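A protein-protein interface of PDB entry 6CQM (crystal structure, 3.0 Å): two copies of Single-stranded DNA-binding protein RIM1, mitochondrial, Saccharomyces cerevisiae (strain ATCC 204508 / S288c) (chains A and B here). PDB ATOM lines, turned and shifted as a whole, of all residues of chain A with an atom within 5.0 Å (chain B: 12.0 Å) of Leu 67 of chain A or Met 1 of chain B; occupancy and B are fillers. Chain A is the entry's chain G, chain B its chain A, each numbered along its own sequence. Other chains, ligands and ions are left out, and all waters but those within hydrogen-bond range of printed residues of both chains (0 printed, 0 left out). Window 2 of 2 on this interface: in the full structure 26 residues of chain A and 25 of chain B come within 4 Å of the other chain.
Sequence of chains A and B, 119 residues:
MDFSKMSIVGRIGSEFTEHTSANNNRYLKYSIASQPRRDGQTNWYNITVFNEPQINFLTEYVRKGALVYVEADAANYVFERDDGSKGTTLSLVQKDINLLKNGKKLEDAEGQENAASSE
The side-chain carboxylate (OD2) of Asp 2 of chain B is in salt-bridge range of the guanidinium group (NH2) of Arg 11 of chain A. The backbone carbonyl oxygen of Phe 3 of chain B sits at hydrogen-bond distance from the backbone NH of Val 9 of chain A (3.0 Å).
N of Val 68 of chain A lies within hydrogen-bond range of O of Gly 10 of chain A (2.9 Å). The backbone carbonyl oxygen (O) of Leu 67 of chain A is in hydrogen-bond range of the backbone NH (N) of Leu 100 of chain A (2.9 Å). The backbone NH (N) of Leu 67 of chain A is in hydrogen-bond range of the backbone carbonyl oxygen (O) of Lys 101 of chain A (2.6 Å).
Among the printed residues, pairs that only touch across the chains: Val 9 of chain A with Met 1 of chain B (3.5 Å), Val 9 of chain A with Asp 2 of chain B (3.3 Å), Gly 10 of chain A with Asp 2 of chain B (3.7 Å), Pro 36 of chain A with Asp 2 of chain B (3.3 Å), Leu 67 of chain A with Met 1 of chain B (3.6 Å) and Leu 67 of chain A with Asp 2 of chain B (3.8 Å).
Val 9 of chain A touches just these residues of chain B: Met 1 (3.5 Å), Asp 2 (3.3 Å) and Phe 3 (3.0 Å). Gly 10 of chain A touches just one residue of chain B: Asp 2. Of the printed residues of chain B, Pro 36 of chain A touches Asp 2. No residue of chain B comes within 4 Å of Ala 66 of chain A. Leu 67 of chain A touches two residues of chain B. Val 68 of chain A touches none of the printed residues of chain B. No residue of chain B comes within 4 Å of Leu 99 of chain A. No residue of chain B comes within 4 Å of Leu 100 of chain A. No residue of chain B comes within 4 Å of Lys 101 of chain A. Asn 102 of chain A touches none of the printed residues of chain B. Met 1 of chain B touches two residues of chain A. Of the printed residues of chain A, Asp 2 of chain B touches Val 9 (3.3 Å), Gly 10 (3.7 Å), Arg 11 (3.8 Å), Pro 36 (3.3 Å) and Leu 67 (3.8 Å). Printed residues of chain A within 4 Å of Phe 3 of chain B: Val 9 (3.0 Å). Ser 4 of chain B touches none of the printed residues of chain A. The nearest printed residue of chain A that does not touch Phe 3 of chain B is Tyr 69 of chain A (4.1 Å).
Hydrophobic or aromatic side chains of chain B within 4 Å of the printed part of chain A: Met 1 and Phe 3.
No position is printed for both chains. Of the 8 pairs that touch across the chains among the printed residues, none has its exchanged pair printed and touching as well.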
ATOM      1  N   VAL A   9     -22.177 -16.485  -3.842  1.00  0.00           N
ATOM      2  CA  VAL A   9     -21.665 -15.384  -3.036  1.00  0.00           C
ATOM      3  C   VAL A   9     -21.305 -15.953  -1.673  1.00  0.00           C
ATOM      4  O   VAL A   9     -22.146 -16.574  -1.010  1.00  0.00           O
ATOM      5  CB  VAL A   9     -22.679 -14.235  -2.910  1.00  0.00           C
ATOM      6  CG1 VAL A   9     -22.456 -13.467  -1.617  1.00  0.00           C
ATOM      7  CG2 VAL A   9     -22.548 -13.298  -4.091  1.00  0.00           C
ATOM      8  N   GLY A  10     -20.059 -15.760  -1.267  1.00  0.00           N
ATOM      9  CA  GLY A  10     -19.617 -16.274   0.011  1.00  0.00           C
ATOM     10  C   GLY A  10     -18.200 -15.845   0.306  1.00  0.00           C
ATOM     11  O   GLY A  10     -17.612 -15.031  -0.408  1.00  0.00           O
ATOM     12  N   ARG A  11     -17.656 -16.412   1.376  1.00  0.00           N
ATOM     13  CA  ARG A  11     -16.307 -16.108   1.824  1.00  0.00           C
ATOM     14  C   ARG A  11     -15.371 -17.244   1.446  1.00  0.00           C
ATOM     15  O   ARG A  11     -15.721 -18.420   1.578  1.00  0.00           O
ATOM     16  CB  ARG A  11     -16.279 -15.878   3.336  1.00  0.00           C
ATOM     17  CG  ARG A  11     -17.178 -14.742   3.800  1.00  0.00           C
ATOM     18  CD  ARG A  11     -17.454 -14.813   5.292  1.00  0.00           C
ATOM     19  NE  ARG A  11     -18.722 -15.476   5.580  1.00  0.00           N
ATOM     20  CZ  ARG A  11     -18.853 -16.780   5.810  1.00  0.00           C
ATOM     21  NH1 ARG A  11     -17.789 -17.571   5.788  1.00  0.00           N
ATOM     22  NH2 ARG A  11     -20.050 -17.291   6.062  1.00  0.00           N
ATOM     23  N   PRO A  36     -26.220 -18.565   3.869  1.00  0.00           N
ATOM     24  CA  PRO A  36     -27.311 -17.609   3.607  1.00  0.00           C
ATOM     25  C   PRO A  36     -27.949 -17.062   4.872  1.00  0.00           C
ATOM     26  O   PRO A  36     -28.201 -15.854   4.959  1.00  0.00           O
ATOM     27  CB  PRO A  36     -28.307 -18.432   2.776  1.00  0.00           C
ATOM     28  CG  PRO A  36     -27.519 -19.608   2.268  1.00  0.00           C
ATOM     29  CD  PRO A  36     -26.518 -19.903   3.336  1.00  0.00           C
ATOM     30  N   GLY A  65     -10.581 -15.475   3.286  1.00  0.00           N
ATOM     31  CA  GLY A  65     -11.682 -14.837   3.975  1.00  0.00           C
ATOM     32  C   GLY A  65     -12.360 -13.731   3.203  1.00  0.00           C
ATOM     33  O   GLY A  65     -13.214 -13.037   3.767  1.00  0.00           O
ATOM     34  N   ALA A  66     -12.014 -13.547   1.933  1.00  0.00           N
ATOM     35  CA  ALA A  66     -12.595 -12.481   1.132  1.00  0.00           C
ATOM     36  C   ALA A  66     -13.998 -12.853   0.670  1.00  0.00           C
ATOM     37  O   ALA A  66     -14.268 -14.004   0.314  1.00  0.00           O
ATOM     38  CB  ALA A  66     -11.712 -12.185  -0.079  1.00  0.00           C
ATOM     39  N   LEU A  67     -14.892 -11.869   0.680  1.00  0.00           N
ATOM     40  CA  LEU A  67     -16.240 -12.051   0.159  1.00  0.00           C
ATOM     41  C   LEU A  67     -16.217 -11.859  -1.352  1.00  0.00           C
ATOM     42  O   LEU A  67     -15.827 -10.793  -1.842  1.00  0.00           O
ATOM     43  CB  LEU A  67     -17.204 -11.067   0.816  1.00  0.00           C
ATOM     44  CG  LEU A  67     -18.676 -11.185   0.421  1.00  0.00           C
ATOM     45  CD1 LEU A  67     -19.269 -12.496   0.921  1.00  0.00           C
ATOM     46  CD2 LEU A  67     -19.460  -9.995   0.949  1.00  0.00           C
ATOM     47  N   VAL A  68     -16.627 -12.888  -2.093  1.00  0.00           N
ATOM     48  CA  VAL A  68     -16.545 -12.882  -3.545  1.00  0.00           C
ATOM     49  C   VAL A  68     -17.886 -13.292  -4.141  1.00  0.00           C
ATOM     50  O   VAL A  68     -18.722 -13.919  -3.487  1.00  0.00           O
ATOM     51  CB  VAL A  68     -15.429 -13.813  -4.068  1.00  0.00           C
ATOM     52  CG1 VAL A  68     -14.064 -13.334  -3.592  1.00  0.00           C
ATOM     53  CG2 VAL A  68     -15.685 -15.246  -3.623  1.00  0.00           C
ATOM     54  N   TYR A  69     -18.078 -12.921  -5.405  1.00  0.00           N
ATOM     55  CA  TYR A  69     -19.202 -13.378  -6.217  1.00  0.00           C
ATOM     56  C   TYR A  69     -18.630 -14.124  -7.414  1.00  0.00           C
ATOM     57  O   TYR A  69     -17.969 -13.524  -8.268  1.00  0.00           O
ATOM     58  CB  TYR A  69     -20.083 -12.211  -6.662  1.00  0.00           C
ATOM     59  CG  TYR A  69     -21.073 -12.582  -7.742  1.00  0.00           C
ATOM     60  CD1 TYR A  69     -22.018 -13.577  -7.531  1.00  0.00           C
ATOM     61  CD2 TYR A  69     -21.068 -11.934  -8.969  1.00  0.00           C
ATOM     62  CE1 TYR A  69     -22.926 -13.921  -8.514  1.00  0.00           C
ATOM     63  CE2 TYR A  69     -21.972 -12.270  -9.959  1.00  0.00           C
ATOM     64  CZ  TYR A  69     -22.899 -13.264  -9.726  1.00  0.00           C
ATOM     65  OH  TYR A  69     -23.803 -13.606 -10.705  1.00  0.00           O
ATOM     66  N   ASN A  98     -15.909 -11.621  -8.879  1.00  0.00           N
ATOM     67  CA  ASN A  98     -15.909 -10.214  -8.496  1.00  0.00           C
ATOM     68  C   ASN A  98     -15.593 -10.127  -7.012  1.00  0.00           C
ATOM     69  O   ASN A  98     -16.276 -10.753  -6.194  1.00  0.00           O
ATOM     70  CB  ASN A  98     -17.256  -9.553  -8.796  1.00  0.00           C
ATOM     71  CG  ASN A  98     -17.246  -8.060  -8.532  1.00  0.00           C
ATOM     72  OD1 ASN A  98     -17.679  -7.603  -7.476  1.00  0.00           O
ATOM     73  ND2 ASN A  98     -16.751  -7.293  -9.497  1.00  0.00           N
ATOM     74  N   LEU A  99     -14.563  -9.358  -6.667  1.00  0.00           N
ATOM     75  CA  LEU A  99     -14.128  -9.236  -5.280  1.00  0.00           C
ATOM     76  C   LEU A  99     -14.970  -8.176  -4.582  1.00  0.00           C
ATOM     77  O   LEU A  99     -14.803  -6.976  -4.828  1.00  0.00           O
ATOM     78  CB  LEU A  99     -12.643  -8.891  -5.216  1.00  0.00           C
ATOM     79  CG  LEU A  99     -12.062  -8.716  -3.812  1.00  0.00           C
ATOM     80  CD1 LEU A  99     -12.282  -9.974  -2.986  1.00  0.00           C
ATOM     81  CD2 LEU A  99     -10.583  -8.369  -3.883  1.00  0.00           C
ATOM     82  N   LEU A 100     -15.874  -8.616  -3.707  1.00  0.00           N
ATOM     83  CA  LEU A 100     -16.726  -7.684  -2.977  1.00  0.00           C
ATOM     84  C   LEU A 100     -15.970  -7.029  -1.827  1.00  0.00           C
ATOM     85  O   LEU A 100     -15.928  -5.798  -1.723  1.00  0.00           O
ATOM     86  CB  LEU A 100     -17.971  -8.409  -2.464  1.00  0.00           C
ATOM     87  CG  LEU A 100     -18.749  -9.199  -3.519  1.00  0.00           C
ATOM     88  CD1 LEU A 100     -19.969  -9.869  -2.909  1.00  0.00           C
ATOM     89  CD2 LEU A 100     -19.153  -8.298  -4.674  1.00  0.00           C
ATOM     90  N   LYS A 101     -15.370  -7.834  -0.955  1.00  0.00           N
ATOM     91  CA  LYS A 101     -14.567  -7.319   0.147  1.00  0.00           C
ATOM     92  C   LYS A 101     -13.456  -8.315   0.436  1.00  0.00           C
ATOM     93  O   LYS A 101     -13.721  -9.511   0.588  1.00  0.00           O
ATOM     94  CB  LYS A 101     -15.420  -7.083   1.398  1.00  0.00           C
ATOM     95  CG  LYS A 101     -14.629  -6.603   2.605  1.00  0.00           C
ATOM     96  CD  LYS A 101     -15.548  -6.216   3.752  1.00  0.00           C
ATOM     97  CE  LYS A 101     -16.411  -7.385   4.195  1.00  0.00           C
ATOM     98  NZ  LYS A 101     -17.318  -7.010   5.314  1.00  0.00           N
ATOM     99  N   ASN A 102     -12.222  -7.824   0.506  1.00  0.00           N
ATOM    100  CA  ASN A 102     -11.081  -8.699   0.705  1.00  0.00           C
ATOM    101  C   ASN A 102     -10.973  -9.115   2.172  1.00  0.00           C
ATOM    102  O   ASN A 102     -11.644  -8.573   3.055  1.00  0.00           O
ATOM    103  CB  ASN A 102      -9.798  -8.016   0.235  1.00  0.00           C
ATOM    104  CG  ASN A 102      -8.804  -8.995  -0.360  1.00  0.00           C
ATOM    105  OD1 ASN A 102      -8.794 -10.175  -0.012  1.00  0.00           O
ATOM    106  ND2 ASN A 102      -7.966  -8.509  -1.269  1.00  0.00           N
ATOM    107  N   MET B   1     -27.618 -12.218   2.230  1.00  0.00           N
ATOM    108  CA  MET B   1     -26.282 -11.886   1.749  1.00  0.00           C
ATOM    109  C   MET B   1     -25.706 -13.006   0.890  1.00  0.00           C
ATOM    110  O   MET B   1     -25.667 -12.905  -0.336  1.00  0.00           O
ATOM    111  CB  MET B   1     -25.345 -11.596   2.922  1.00  0.00           C
ATOM    112  CG  MET B   1     -24.956 -10.133   3.054  1.00  0.00           C
ATOM    113  SD  MET B   1     -24.350  -9.443   1.502  1.00  0.00           S
ATOM    114  CE  MET B   1     -23.003 -10.564   1.136  1.00  0.00           C
ATOM    115  N   ASP B   2     -25.250 -14.071   1.542  1.00  0.00           N
ATOM    116  CA  ASP B   2     -24.711 -15.212   0.820  1.00  0.00           C
ATOM    117  C   ASP B   2     -25.832 -16.014   0.169  1.00  0.00           C
ATOM    118  O   ASP B   2     -26.953 -16.088   0.679  1.00  0.00           O
ATOM    119  CB  ASP B   2     -23.905 -16.110   1.759  1.00  0.00           C
ATOM    120  CG  ASP B   2     -22.643 -15.443   2.266  1.00  0.00           C
ATOM    121  OD1 ASP B   2     -22.452 -14.240   1.990  1.00  0.00           O
ATOM    122  OD2 ASP B   2     -21.840 -16.122   2.940  1.00  0.00           O
ATOM    123  N   PHE B   3     -25.516 -16.615  -0.975  1.00  0.00           N
ATOM    124  CA  PHE B   3     -26.460 -17.471  -1.678  1.00  0.00           C
ATOM    125  C   PHE B   3     -25.684 -18.355  -2.641  1.00  0.00           C
ATOM    126  O   PHE B   3     -24.517 -18.096  -2.949  1.00  0.00           O
ATOM    127  CB  PHE B   3     -27.519 -16.656  -2.431  1.00  0.00           C
ATOM    128  CG  PHE B   3     -26.999 -15.976  -3.667  1.00  0.00           C
ATOM    129  CD1 PHE B   3     -26.346 -14.759  -3.583  1.00  0.00           C
ATOM    130  CD2 PHE B   3     -27.171 -16.552  -4.915  1.00  0.00           C
ATOM    131  CE1 PHE B   3     -25.871 -14.132  -4.719  1.00  0.00           C
ATOM    132  CE2 PHE B   3     -26.696 -15.931  -6.054  1.00  0.00           C
ATOM    133  CZ  PHE B   3     -26.045 -14.719  -5.955  1.00  0.00           C
ATOM    134  N   SER B   4     -26.355 -19.402  -3.119  1.00  0.00           N
ATOM    135  CA  SER B   4     -25.755 -20.322  -4.085  1.00  0.00           C
ATOM    136  C   SER B   4     -26.892 -20.877  -4.945  1.00  0.00           C
ATOM    137  O   SER B   4     -27.514 -21.882  -4.598  1.00  0.00           O
ATOM    138  CB  SER B   4     -24.975 -21.429  -3.393  1.00  0.00           C
ATOM    139  OG  SER B   4     -25.815 -22.199  -2.551  1.00  0.00           O
ATOM    140  N   LYS B   5     -27.153 -20.205  -6.061  1.00  0.00           N
ATOM    141  CA  LYS B   5     -28.212 -20.581  -6.981  1.00  0.00           C
ATOM    142  C   LYS B   5     -27.613 -21.181  -8.248  1.00  0.00           C
ATOM    143  O   LYS B   5     -26.492 -20.845  -8.643  1.00  0.00           O
ATOM    144  CB  LYS B   5     -29.085 -19.369  -7.331  1.00  0.00           C
ATOM    145  CG  LYS B   5     -30.526 -19.711  -7.672  1.00  0.00           C
ATOM    146  CD  LYS B   5     -31.380 -18.458  -7.798  1.00  0.00           C
ATOM    147  CE  LYS B   5     -32.862 -18.788  -7.716  1.00  0.00           C
ATOM    148  NZ  LYS B   5     -33.711 -17.565  -7.750  1.00  0.00           N
ATOM    149  N   ASP B  73     -32.185 -23.223  -5.804  1.00  0.00           N
ATOM    150  CA  ASP B  73     -31.223 -22.855  -4.773  1.00  0.00           C
ATOM    151  C   ASP B  73     -30.385 -24.078  -4.420  1.00  0.00           C
ATOM    152  O   ASP B  73     -30.928 -25.118  -4.031  1.00  0.00           O
ATOM    153  CB  ASP B  73     -31.936 -22.314  -3.536  1.00  0.00           C
ATOM    154  CG  ASP B  73     -32.550 -20.947  -3.765  1.00  0.00           C
ATOM    155  OD1 ASP B  73     -32.389 -20.397  -4.875  1.00  0.00           O
ATOM    156  OD2 ASP B  73     -33.195 -20.421  -2.833  1.00  0.00           O
ATOM    157  N   ALA B  74     -29.069 -23.956  -4.558  1.00  0.00           N
ATOM    158  CA  ALA B  74     -28.166 -25.068  -4.309  1.00  0.00           C
ATOM    159  C   ALA B  74     -27.711 -25.080  -2.855  1.00  0.00           C
ATOM    160  O   ALA B  74     -27.413 -24.033  -2.274  1.00  0.00           O
ATOM    161  CB  ALA B  74     -26.950 -24.992  -5.234  1.00  0.00           C
